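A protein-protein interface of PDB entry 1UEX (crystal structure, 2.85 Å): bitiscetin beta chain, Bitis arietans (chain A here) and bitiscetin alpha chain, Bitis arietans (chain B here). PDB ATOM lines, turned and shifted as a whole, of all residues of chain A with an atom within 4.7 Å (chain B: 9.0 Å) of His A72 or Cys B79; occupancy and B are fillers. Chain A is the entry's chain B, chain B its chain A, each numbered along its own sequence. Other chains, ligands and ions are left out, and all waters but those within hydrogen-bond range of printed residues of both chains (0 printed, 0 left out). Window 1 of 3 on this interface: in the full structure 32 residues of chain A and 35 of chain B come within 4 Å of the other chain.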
ATOM      1  N   SER A  71     -10.788   5.939  -8.401  1.00  0.00           N
ATOM      2  CA  SER A  71      -9.736   5.352  -7.579  1.00  0.00           C
ATOM      3  C   SER A  71      -9.288   6.392  -6.580  1.00  0.00           C
ATOM      4  O   SER A  71      -9.749   7.534  -6.607  1.00  0.00           O
ATOM      5  CB  SER A  71      -8.532   4.953  -8.427  1.00  0.00           C
ATOM      6  OG  SER A  71      -7.588   6.010  -8.471  1.00  0.00           O
ATOM      7  N   HIS A  72      -8.369   5.996  -5.709  1.00  0.00           N
ATOM      8  CA  HIS A  72      -7.859   6.896  -4.695  1.00  0.00           C
ATOM      9  C   HIS A  72      -6.897   6.161  -3.789  1.00  0.00           C
ATOM     10  O   HIS A  72      -6.798   4.936  -3.830  1.00  0.00           O
ATOM     11  CB  HIS A  72      -9.011   7.450  -3.852  1.00  0.00           C
ATOM     12  CG  HIS A  72      -9.701   6.415  -3.021  1.00  0.00           C
ATOM     13  ND1 HIS A  72      -9.104   5.815  -1.929  1.00  0.00           N
ATOM     14  CD2 HIS A  72     -10.928   5.853  -3.130  1.00  0.00           C
ATOM     15  CE1 HIS A  72      -9.932   4.932  -1.409  1.00  0.00           C
ATOM     16  NE2 HIS A  72     -11.047   4.933  -2.118  1.00  0.00           N
ATOM     17  N   PHE A  73      -6.187   6.936  -2.978  1.00  0.00           N
ATOM     18  CA  PHE A  73      -5.239   6.407  -2.014  1.00  0.00           C
ATOM     19  C   PHE A  73      -5.851   6.725  -0.661  1.00  0.00           C
ATOM     20  O   PHE A  73      -6.804   7.505  -0.575  1.00  0.00           O
ATOM     21  CB  PHE A  73      -3.881   7.101  -2.156  1.00  0.00           C
ATOM     22  CG  PHE A  73      -3.227   6.878  -3.491  1.00  0.00           C
ATOM     23  CD1 PHE A  73      -3.829   7.344  -4.662  1.00  0.00           C
ATOM     24  CD2 PHE A  73      -2.013   6.202  -3.582  1.00  0.00           C
ATOM     25  CE1 PHE A  73      -3.234   7.134  -5.910  1.00  0.00           C
ATOM     26  CE2 PHE A  73      -1.407   5.987  -4.822  1.00  0.00           C
ATOM     27  CZ  PHE A  73      -2.019   6.456  -5.988  1.00  0.00           C
ATOM     28  N   TRP A  74      -5.319   6.130   0.397  1.00  0.00           N
ATOM     29  CA  TRP A  74      -5.867   6.388   1.716  1.00  0.00           C
ATOM     30  C   TRP A  74      -5.478   7.745   2.296  1.00  0.00           C
ATOM     31  O   TRP A  74      -6.276   8.366   2.995  1.00  0.00           O
ATOM     32  CB  TRP A  74      -5.488   5.258   2.676  1.00  0.00           C
ATOM     33  CG  TRP A  74      -6.240   3.987   2.399  1.00  0.00           C
ATOM     34  CD1 TRP A  74      -5.708   2.777   2.076  1.00  0.00           C
ATOM     35  CD2 TRP A  74      -7.665   3.813   2.394  1.00  0.00           C
ATOM     36  NE1 TRP A  74      -6.707   1.860   1.867  1.00  0.00           N
ATOM     37  CE2 TRP A  74      -7.919   2.469   2.056  1.00  0.00           C
ATOM     38  CE3 TRP A  74      -8.752   4.664   2.644  1.00  0.00           C
ATOM     39  CZ2 TRP A  74      -9.215   1.950   1.958  1.00  0.00           C
ATOM     40  CZ3 TRP A  74     -10.045   4.147   2.547  1.00  0.00           C
ATOM     41  CH2 TRP A  74     -10.261   2.801   2.207  1.00  0.00           C
ATOM     42  N   ILE A  76      -5.737  10.298   1.206  1.00  0.00           N
ATOM     43  CA  ILE A  76      -6.535  11.279   0.483  1.00  0.00           C
ATOM     44  C   ILE A  76      -7.896  11.383   1.146  1.00  0.00           C
ATOM     45  O   ILE A  76      -8.577  12.402   1.046  1.00  0.00           O
ATOM     46  CB  ILE A  76      -6.744  10.876  -0.997  1.00  0.00           C
ATOM     47  CG1 ILE A  76      -5.394  10.612  -1.669  1.00  0.00           C
ATOM     48  CG2 ILE A  76      -7.471  11.990  -1.734  1.00  0.00           C
ATOM     49  CD1 ILE A  76      -4.483  11.827  -1.720  1.00  0.00           C
ATOM     50  N   CYS A  77      -8.280  10.313   1.830  1.00  0.00           N
ATOM     51  CA  CYS A  77      -9.563  10.255   2.512  1.00  0.00           C
ATOM     52  C   CYS A  77      -9.523  10.930   3.876  1.00  0.00           C
ATOM     53  O   CYS A  77      -8.453  11.118   4.454  1.00  0.00           O
ATOM     54  CB  CYS A  77      -9.979   8.797   2.682  1.00  0.00           C
ATOM     55  SG  CYS A  77      -9.917   7.877   1.120  1.00  0.00           S
ATOM     56  N   PRO A  78     -10.699  11.304   4.405  1.00  0.00           N
ATOM     57  CA  PRO A  78     -10.833  11.958   5.708  1.00  0.00           C
ATOM     58  C   PRO A  78     -10.895  10.926   6.843  1.00  0.00           C
ATOM     59  O   PRO A  78     -11.891  10.831   7.557  1.00  0.00           O
ATOM     60  CB  PRO A  78     -12.139  12.724   5.560  1.00  0.00           C
ATOM     61  CG  PRO A  78     -12.963  11.764   4.765  1.00  0.00           C
ATOM     62  CD  PRO A  78     -11.993  11.293   3.697  1.00  0.00           C
ATOM     63  N   PRO A  96      -3.062   2.221  -4.045  1.00  0.00           N
ATOM     64  CA  PRO A  96      -4.362   2.821  -4.361  1.00  0.00           C
ATOM     65  C   PRO A  96      -5.491   1.817  -4.551  1.00  0.00           C
ATOM     66  O   PRO A  96      -5.261   0.656  -4.884  1.00  0.00           O
ATOM     67  CB  PRO A  96      -4.075   3.576  -5.649  1.00  0.00           C
ATOM     68  CG  PRO A  96      -3.172   2.609  -6.359  1.00  0.00           C
ATOM     69  CD  PRO A  96      -2.213   2.159  -5.251  1.00  0.00           C
ATOM     70  N   ILE A  97      -6.714   2.285  -4.341  1.00  0.00           N
ATOM     71  CA  ILE A  97      -7.890   1.449  -4.519  1.00  0.00           C
ATOM     72  C   ILE A  97      -8.414   1.778  -5.907  1.00  0.00           C
ATOM     73  O   ILE A  97      -8.345   2.924  -6.341  1.00  0.00           O
ATOM     74  CB  ILE A  97      -8.994   1.770  -3.478  1.00  0.00           C
ATOM     75  CG1 ILE A  97      -8.501   1.444  -2.069  1.00  0.00           C
ATOM     76  CG2 ILE A  97     -10.260   0.979  -3.787  1.00  0.00           C
ATOM     77  CD1 ILE A  97      -7.400   2.352  -1.573  1.00  0.00           C
ATOM     78  N   PHE A  99     -11.603   0.738  -9.035  1.00  0.00           N
ATOM     79  CA  PHE A  99     -12.941   0.182  -9.185  1.00  0.00           C
ATOM     80  C   PHE A  99     -13.289  -0.431 -10.533  1.00  0.00           C
ATOM     81  O   PHE A  99     -12.956   0.092 -11.598  1.00  0.00           O
ATOM     82  CB  PHE A  99     -14.006   1.236  -8.852  1.00  0.00           C
ATOM     83  CG  PHE A  99     -14.144   1.519  -7.390  1.00  0.00           C
ATOM     84  CD1 PHE A  99     -13.201   2.299  -6.727  1.00  0.00           C
ATOM     85  CD2 PHE A  99     -15.204   0.982  -6.668  1.00  0.00           C
ATOM     86  CE1 PHE A  99     -13.308   2.543  -5.361  1.00  0.00           C
ATOM     87  CE2 PHE A  99     -15.323   1.216  -5.301  1.00  0.00           C
ATOM     88  CZ  PHE A  99     -14.372   1.999  -4.647  1.00  0.00           C
ATOM     89  N   ARG B  71     -12.148   5.263  11.038  1.00  0.00           N
ATOM     90  CA  ARG B  71     -13.167   5.145   9.997  1.00  0.00           C
ATOM     91  C   ARG B  71     -13.040   6.248   8.955  1.00  0.00           C
ATOM     92  O   ARG B  71     -12.238   7.168   9.109  1.00  0.00           O
ATOM     93  CB  ARG B  71     -14.577   5.167  10.599  1.00  0.00           C
ATOM     94  CG  ARG B  71     -15.004   6.488  11.226  1.00  0.00           C
ATOM     95  CD  ARG B  71     -16.436   6.816  10.820  1.00  0.00           C
ATOM     96  NE  ARG B  71     -17.353   5.699  11.052  1.00  0.00           N
ATOM     97  CZ  ARG B  71     -18.493   5.514  10.388  1.00  0.00           C
ATOM     98  NH1 ARG B  71     -18.865   6.368   9.441  1.00  0.00           N
ATOM     99  NH2 ARG B  71     -19.267   4.473  10.672  1.00  0.00           N
ATOM    100  N   ASP B  72     -13.838   6.148   7.898  1.00  0.00           N
ATOM    101  CA  ASP B  72     -13.819   7.128   6.813  1.00  0.00           C
ATOM    102  C   ASP B  72     -15.010   8.080   6.939  1.00  0.00           C
ATOM    103  O   ASP B  72     -16.147   7.700   6.670  1.00  0.00           O
ATOM    104  CB  ASP B  72     -13.866   6.395   5.464  1.00  0.00           C
ATOM    105  CG  ASP B  72     -13.603   7.310   4.278  1.00  0.00           C
ATOM    106  OD1 ASP B  72     -13.666   6.824   3.129  1.00  0.00           O
ATOM    107  OD2 ASP B  72     -13.332   8.510   4.490  1.00  0.00           O
ATOM    108  N   GLU B  73     -14.739   9.316   7.350  1.00  0.00           N
ATOM    109  CA  GLU B  73     -15.780  10.329   7.525  1.00  0.00           C
ATOM    110  C   GLU B  73     -16.516  10.635   6.224  1.00  0.00           C
ATOM    111  O   GLU B  73     -17.639  11.133   6.246  1.00  0.00           O
ATOM    112  CB  GLU B  73     -15.170  11.635   8.051  1.00  0.00           C
ATOM    113  CG  GLU B  73     -14.386  11.517   9.345  1.00  0.00           C
ATOM    114  CD  GLU B  73     -15.268  11.260  10.544  1.00  0.00           C
ATOM    115  OE1 GLU B  73     -15.971  10.226  10.550  1.00  0.00           O
ATOM    116  OE2 GLU B  73     -15.256  12.090  11.481  1.00  0.00           O
ATOM    117  N   SER B  74     -15.872  10.348   5.097  1.00  0.00           N
ATOM    118  CA  SER B  74     -16.440  10.616   3.780  1.00  0.00           C
ATOM    119  C   SER B  74     -17.953  10.507   3.704  1.00  0.00           C
ATOM    120  O   SER B  74     -18.542   9.523   4.152  1.00  0.00           O
ATOM    121  CB  SER B  74     -15.819   9.688   2.741  1.00  0.00           C
ATOM    122  OG  SER B  74     -14.435   9.942   2.617  1.00  0.00           O
ATOM    123  N   LYS B  75     -18.573  11.531   3.127  1.00  0.00           N
ATOM    124  CA  LYS B  75     -20.023  11.579   2.967  1.00  0.00           C
ATOM    125  C   LYS B  75     -20.460  10.557   1.917  1.00  0.00           C
ATOM    126  O   LYS B  75     -21.580  10.049   1.959  1.00  0.00           O
ATOM    127  CB  LYS B  75     -20.454  12.981   2.513  1.00  0.00           C
ATOM    128  CG  LYS B  75     -20.020  14.134   3.419  1.00  0.00           C
ATOM    129  CD  LYS B  75     -20.859  14.229   4.687  1.00  0.00           C
ATOM    130  CE  LYS B  75     -20.512  15.488   5.478  1.00  0.00           C
ATOM    131  NZ  LYS B  75     -21.299  15.612   6.737  1.00  0.00           N
ATOM    132  N   THR B  76     -19.552  10.263   0.985  1.00  0.00           N
ATOM    133  CA  THR B  76     -19.789   9.327  -0.115  1.00  0.00           C
ATOM    134  C   THR B  76     -19.461   7.867   0.197  1.00  0.00           C
ATOM    135  O   THR B  76     -18.720   7.568   1.139  1.00  0.00           O
ATOM    136  CB  THR B  76     -18.971   9.735  -1.353  1.00  0.00           C
ATOM    137  OG1 THR B  76     -17.593   9.884  -0.988  1.00  0.00           O
ATOM    138  CG2 THR B  76     -19.475  11.049  -1.913  1.00  0.00           C
ATOM    139  N   GLN B  77     -20.019   6.962  -0.610  1.00  0.00           N
ATOM    140  CA  GLN B  77     -19.789   5.528  -0.451  1.00  0.00           C
ATOM    141  C   GLN B  77     -18.288   5.270  -0.431  1.00  0.00           C
ATOM    142  O   GLN B  77     -17.745   4.863   0.594  1.00  0.00           O
ATOM    143  CB  GLN B  77     -20.466   4.753  -1.583  1.00  0.00           C
ATOM    144  CG  GLN B  77     -21.983   4.759  -1.481  1.00  0.00           C
ATOM    145  CD  GLN B  77     -22.661   3.949  -2.569  1.00  0.00           C
ATOM    146  OE1 GLN B  77     -22.319   2.790  -2.802  1.00  0.00           O
ATOM    147  NE2 GLN B  77     -23.638   4.552  -3.234  1.00  0.00           N
ATOM    148  N   GLN B  78     -17.616   5.489  -1.557  1.00  0.00           N
ATOM    149  CA  GLN B  78     -16.168   5.337  -1.579  1.00  0.00           C
ATOM    150  C   GLN B  78     -15.638   6.766  -1.387  1.00  0.00           C
ATOM    151  O   GLN B  78     -16.403   7.724  -1.467  1.00  0.00           O
ATOM    152  CB  GLN B  78     -15.684   4.677  -2.884  1.00  0.00           C
ATOM    153  CG  GLN B  78     -16.149   5.314  -4.172  1.00  0.00           C
ATOM    154  CD  GLN B  78     -15.438   6.607  -4.454  1.00  0.00           C
ATOM    155  OE1 GLN B  78     -16.066   7.638  -4.665  1.00  0.00           O
ATOM    156  NE2 GLN B  78     -14.117   6.561  -4.465  1.00  0.00           N
ATOM    157  N   CYS B  79     -14.346   6.923  -1.128  1.00  0.00           N
ATOM    158  CA  CYS B  79     -13.812   8.254  -0.853  1.00  0.00           C
ATOM    159  C   CYS B  79     -13.251   9.139  -1.976  1.00  0.00           C
ATOM    160  O   CYS B  79     -12.887  10.289  -1.725  1.00  0.00           O
ATOM    161  CB  CYS B  79     -12.792   8.137   0.279  1.00  0.00           C
ATOM    162  SG  CYS B  79     -11.200   8.946  -0.030  1.00  0.00           S
ATOM    163  N   SER B  80     -13.187   8.635  -3.203  1.00  0.00           N
ATOM    164  CA  SER B  80     -12.685   9.447  -4.306  1.00  0.00           C
ATOM    165  C   SER B  80     -13.719  10.521  -4.643  1.00  0.00           C
ATOM    166  O   SER B  80     -14.846  10.210  -5.023  1.00  0.00           O
ATOM    167  CB  SER B  80     -12.415   8.573  -5.532  1.00  0.00           C
ATOM    168  OG  SER B  80     -11.947   9.342  -6.626  1.00  0.00           O
ATOM    169  N   PRO B  81     -13.347  11.804  -4.501  1.00  0.00           N
ATOM    170  CA  PRO B  81     -14.243  12.926  -4.788  1.00  0.00           C
ATOM    171  C   PRO B  81     -14.374  13.298  -6.261  1.00  0.00           C
ATOM    172  O   PRO B  81     -15.398  13.838  -6.675  1.00  0.00           O
ATOM    173  CB  PRO B  81     -13.638  14.053  -3.972  1.00  0.00           C
ATOM    174  CG  PRO B  81     -12.187  13.793  -4.123  1.00  0.00           C
ATOM    175  CD  PRO B  81     -12.094  12.292  -3.894  1.00  0.00           C
ATOM    176  N   GLN B  82     -13.343  13.017  -7.049  1.00  0.00           N
ATOM    177  CA  GLN B  82     -13.372  13.347  -8.471  1.00  0.00           C
ATOM    178  C   GLN B  82     -13.119  12.107  -9.322  1.00  0.00           C
ATOM    179  O   GLN B  82     -12.467  11.160  -8.870  1.00  0.00           O
ATOM    180  CB  GLN B  82     -12.292  14.387  -8.789  1.00  0.00           C
ATOM    181  CG  GLN B  82     -12.759  15.594  -9.595  1.00  0.00           C
ATOM    182  CD  GLN B  82     -13.558  16.588  -8.759  1.00  0.00           C
ATOM    183  OE1 GLN B  82     -13.097  17.045  -7.709  1.00  0.00           O
ATOM    184  NE2 GLN B  82     -14.756  16.932  -9.225  1.00  0.00           N
ATOM    185  N   THR B  84     -11.750  10.417 -13.146  1.00  0.00           N
ATOM    186  CA  THR B  84     -10.557  10.651 -13.951  1.00  0.00           C
ATOM    187  C   THR B  84     -10.820  11.708 -15.011  1.00  0.00           C
ATOM    188  O   THR B  84      -9.892  12.367 -15.472  1.00  0.00           O
ATOM    189  CB  THR B  84     -10.085   9.374 -14.660  1.00  0.00           C
ATOM    190  OG1 THR B  84     -11.176   8.801 -15.395  1.00  0.00           O
ATOM    191  CG2 THR B  84      -9.571   8.376 -13.654  1.00  0.00           C
ATOM    192  N   VAL B  89     -17.914  13.279  -8.208  1.00  0.00           N
ATOM    193  CA  VAL B  89     -18.568  12.026  -7.856  1.00  0.00           C
ATOM    194  C   VAL B  89     -19.862  12.334  -7.119  1.00  0.00           C
ATOM    195  O   VAL B  89     -19.871  12.556  -5.910  1.00  0.00           O
ATOM    196  CB  VAL B  89     -17.683  11.144  -6.959  1.00  0.00           C
ATOM    197  CG1 VAL B  89     -18.349   9.788  -6.762  1.00  0.00           C
ATOM    198  CG2 VAL B  89     -16.308  10.973  -7.587  1.00  0.00           C
ATOM    199  N   GLU B  92     -23.363   7.163  -6.930  1.00  0.00           N
ATOM    200  CA  GLU B  92     -22.489   6.024  -6.636  1.00  0.00           C
ATOM    201  C   GLU B  92     -23.268   4.718  -6.648  1.00  0.00           C
ATOM    202  O   GLU B  92     -24.497   4.719  -6.615  1.00  0.00           O
ATOM    203  CB  GLU B  92     -21.798   6.191  -5.281  1.00  0.00           C
ATOM    204  CG  GLU B  92     -20.688   7.228  -5.260  1.00  0.00           C
ATOM    205  CD  GLU B  92     -20.117   7.425  -3.872  1.00  0.00           C
ATOM    206  OE1 GLU B  92     -20.905   7.748  -2.959  1.00  0.00           O
ATOM    207  OE2 GLU B  92     -18.893   7.260  -3.689  1.00  0.00           O
ATOM    208  N   VAL B  94     -21.438   1.571  -5.299  1.00  0.00           N
ATOM    209  CA  VAL B  94     -20.513   0.620  -4.704  1.00  0.00           C
ATOM    210  C   VAL B  94     -21.333  -0.485  -4.059  1.00  0.00           C
ATOM    211  O   VAL B  94     -22.170  -0.224  -3.198  1.00  0.00           O
ATOM    212  CB  VAL B  94     -19.637   1.283  -3.618  1.00  0.00           C
ATOM    213  CG1 VAL B  94     -18.504   0.355  -3.234  1.00  0.00           C
ATOM    214  CG2 VAL B  94     -19.093   2.609  -4.113  1.00  0.00           C
ATOM    215  N   PRO B  97     -19.634  -0.523   0.339  1.00  0.00           N
ATOM    216  CA  PRO B  97     -18.534   0.340   0.767  1.00  0.00           C
ATOM    217  C   PRO B  97     -17.916  -0.113   2.088  1.00  0.00           C
ATOM    218  O   PRO B  97     -18.600  -0.636   2.966  1.00  0.00           O
ATOM    219  CB  PRO B  97     -19.191   1.722   0.849  1.00  0.00           C
ATOM    220  CG  PRO B  97     -20.617   1.408   1.134  1.00  0.00           C
ATOM    221  CD  PRO B  97     -20.891   0.235   0.239  1.00  0.00           C
ATOM    222  N   THR B  98     -16.608   0.079   2.212  1.00  0.00           N
ATOM    223  CA  THR B  98     -15.878  -0.296   3.414  1.00  0.00           C
ATOM    224  C   THR B  98     -15.291   0.974   4.010  1.00  0.00           C
ATOM    225  O   THR B  98     -14.286   1.484   3.528  1.00  0.00           O
ATOM    226  CB  THR B  98     -14.742  -1.275   3.073  1.00  0.00           C
ATOM    227  OG1 THR B  98     -14.045  -0.803   1.916  1.00  0.00           O
ATOM    228  CG2 THR B  98     -15.292  -2.655   2.786  1.00  0.00           C
ATOM    229  N   LYS B  99     -15.911   1.480   5.067  1.00  0.00           N
ATOM    230  CA  LYS B  99     -15.444   2.719   5.667  1.00  0.00           C
ATOM    231  C   LYS B  99     -14.999   2.608   7.124  1.00  0.00           C
ATOM    232  O   LYS B  99     -14.754   3.620   7.788  1.00  0.00           O
ATOM    233  CB  LYS B  99     -16.540   3.771   5.513  1.00  0.00           C
ATOM    234  CG  LYS B  99     -17.044   3.861   4.076  1.00  0.00           C
ATOM    235  CD  LYS B  99     -18.158   4.869   3.901  1.00  0.00           C
ATOM    236  CE  LYS B  99     -17.725   6.249   4.363  1.00  0.00           C
ATOM    237  NZ  LYS B  99     -16.442   6.692   3.743  1.00  0.00           N
ATOM    238  N   PHE B 101     -12.134   0.658   9.586  1.00  0.00           N
ATOM    239  CA  PHE B 101     -10.915  -0.137   9.610  1.00  0.00           C
ATOM    240  C   PHE B 101     -10.778  -1.038  10.826  1.00  0.00           C
ATOM    241  O   PHE B 101     -11.391  -0.803  11.866  1.00  0.00           O
ATOM    242  CB  PHE B 101      -9.685   0.765   9.520  1.00  0.00           C
ATOM    243  CG  PHE B 101      -9.637   1.580   8.271  1.00  0.00           C
ATOM    244  CD1 PHE B 101     -10.479   2.676   8.112  1.00  0.00           C
ATOM    245  CD2 PHE B 101      -8.784   1.230   7.233  1.00  0.00           C
ATOM    246  CE1 PHE B 101     -10.472   3.414   6.934  1.00  0.00           C
ATOM    247  CE2 PHE B 101      -8.770   1.961   6.049  1.00  0.00           C
ATOM    248  CZ  PHE B 101      -9.617   3.053   5.899  1.00  0.00           C
ATOM    249  N   ASP B 114      -9.535  -1.780   5.876  1.00  0.00           N
ATOM    250  CA  ASP B 114     -10.847  -1.171   5.904  1.00  0.00           C
ATOM    251  C   ASP B 114     -11.776  -2.375   5.790  1.00  0.00           C
ATOM    252  O   ASP B 114     -11.389  -3.418   5.255  1.00  0.00           O
ATOM    253  CB  ASP B 114     -11.035  -0.222   4.719  1.00  0.00           C
ATOM    254  CG  ASP B 114     -10.731  -0.881   3.394  1.00  0.00           C
ATOM    255  OD1 ASP B 114      -9.584  -1.335   3.199  1.00  0.00           O
ATOM    256  OD2 ASP B 114     -11.640  -0.943   2.547  1.00  0.00           O
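Printed residues of chain B that touch a printed residue of chain A: Arg B71, Asp B72, Glu B73, Ser B74, Gln B78, Cys B79, Ser B80, Val B94, Phe B101 and Asp B114. Hydrophobic or aromatic side chains of chain B that line the printed part of chain A: Val B94 and Phe B101. Of the 10 printed residues of chain A, 6 touch a printed residue of chain B. Printed residues of chain A that touch a printed residue of chain B: Ser A71, His A72, Trp A74, Cys A77, Pro A78 and Phe A99. Hydrophobic or aromatic side chains of chain A within 4 Å of the printed part of chain B: His A72, Trp A74, Pro A78 and Phe A99. Among the printed residues, 14 pairs touch across the chains. Among the printed residues, no Asp or Glu carboxylate lies within 4 Å of a Lys or Arg side-chain nitrogen of the other chain.
The backbone carbonyl oxygen (O) of Pro A78 sits close to the backbone NH (N) of Glu B73 (3.2 Å). SG of Cys B79 forms a disulfide with SG of Cys A77, at 2.0 Å. O of Ser A71 lies within hydrogen-bond range of OG of Ser B80 (2.8 Å).
Of chain B, only Ser B80 (2.8 Å) comes within 4 Å of Ser A71. Of chain B, only Gln B78 (3.5 Å), Cys B79 (3.98 Å) and Ser B80 (3.6 Å) come within 4 Å of His A72. Of the printed residues of chain B, Trp A74 touches Phe B101 and Asp B114. Printed residues of chain B within 4 Å of Pro A78: Arg B71, Asp B72, Glu B73 and Ser B74. No residue of chain B comes within 4 Å of Ile A97. Of the printed residues of chain A, Ser B74 touches Pro A78 (3.0 Å). Of the printed residues of chain A, Gln B78 touches His A72 (3.5 Å) and Phe A99 (3.5 Å). Cys B79 touches two residues of chain A. Printed residues of chain A within 4 Å of Phe B101: Trp A74. The nearest residue of chain A that does not touch Cys B79 is Ile A76 (4.3 Å).
NZ of Lys B99 is in salt-bridge range of OD1 of Asp B72 (2.8 Å). The side-chain hydroxyl (OG1) of Thr B76 sits at hydrogen-bond distance from the backbone carbonyl oxygen (O) of Gln B78 (2.5 Å). NE2 of Gln B78 sits close to N of Ser B80. OE1 of Gln B78 sits close to OE2 of Glu B92 (3.0 Å). The side-chain hydroxyl (OG) of Ser B80 sits at hydrogen-bond distance from the backbone carbonyl oxygen (O) of Gln B82 (2.9 Å). SG of Cys A77 lies within hydrogen-bond range of ND1 of His A72, at 3.8 Å.
His A72 touches Gln B78 (CD2 to NE2, 3.5 Å). His A72 touches Cys B79 (NE2 to N, 3.98 Å). Ser B80 touches His A72 (N to CD2, 3.6 Å). Trp A74 touches Asp B114. CB of Cys A77 touches OD2 of Asp B72, 3.8 Å away. Arg B71 touches Pro A78. OD2 of Asp B72 touches CD of Pro A78 (3.2 Å). Pro A78 touches Ser B74. Phe A99 touches Gln B78. Phe A99 touches Val B94.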
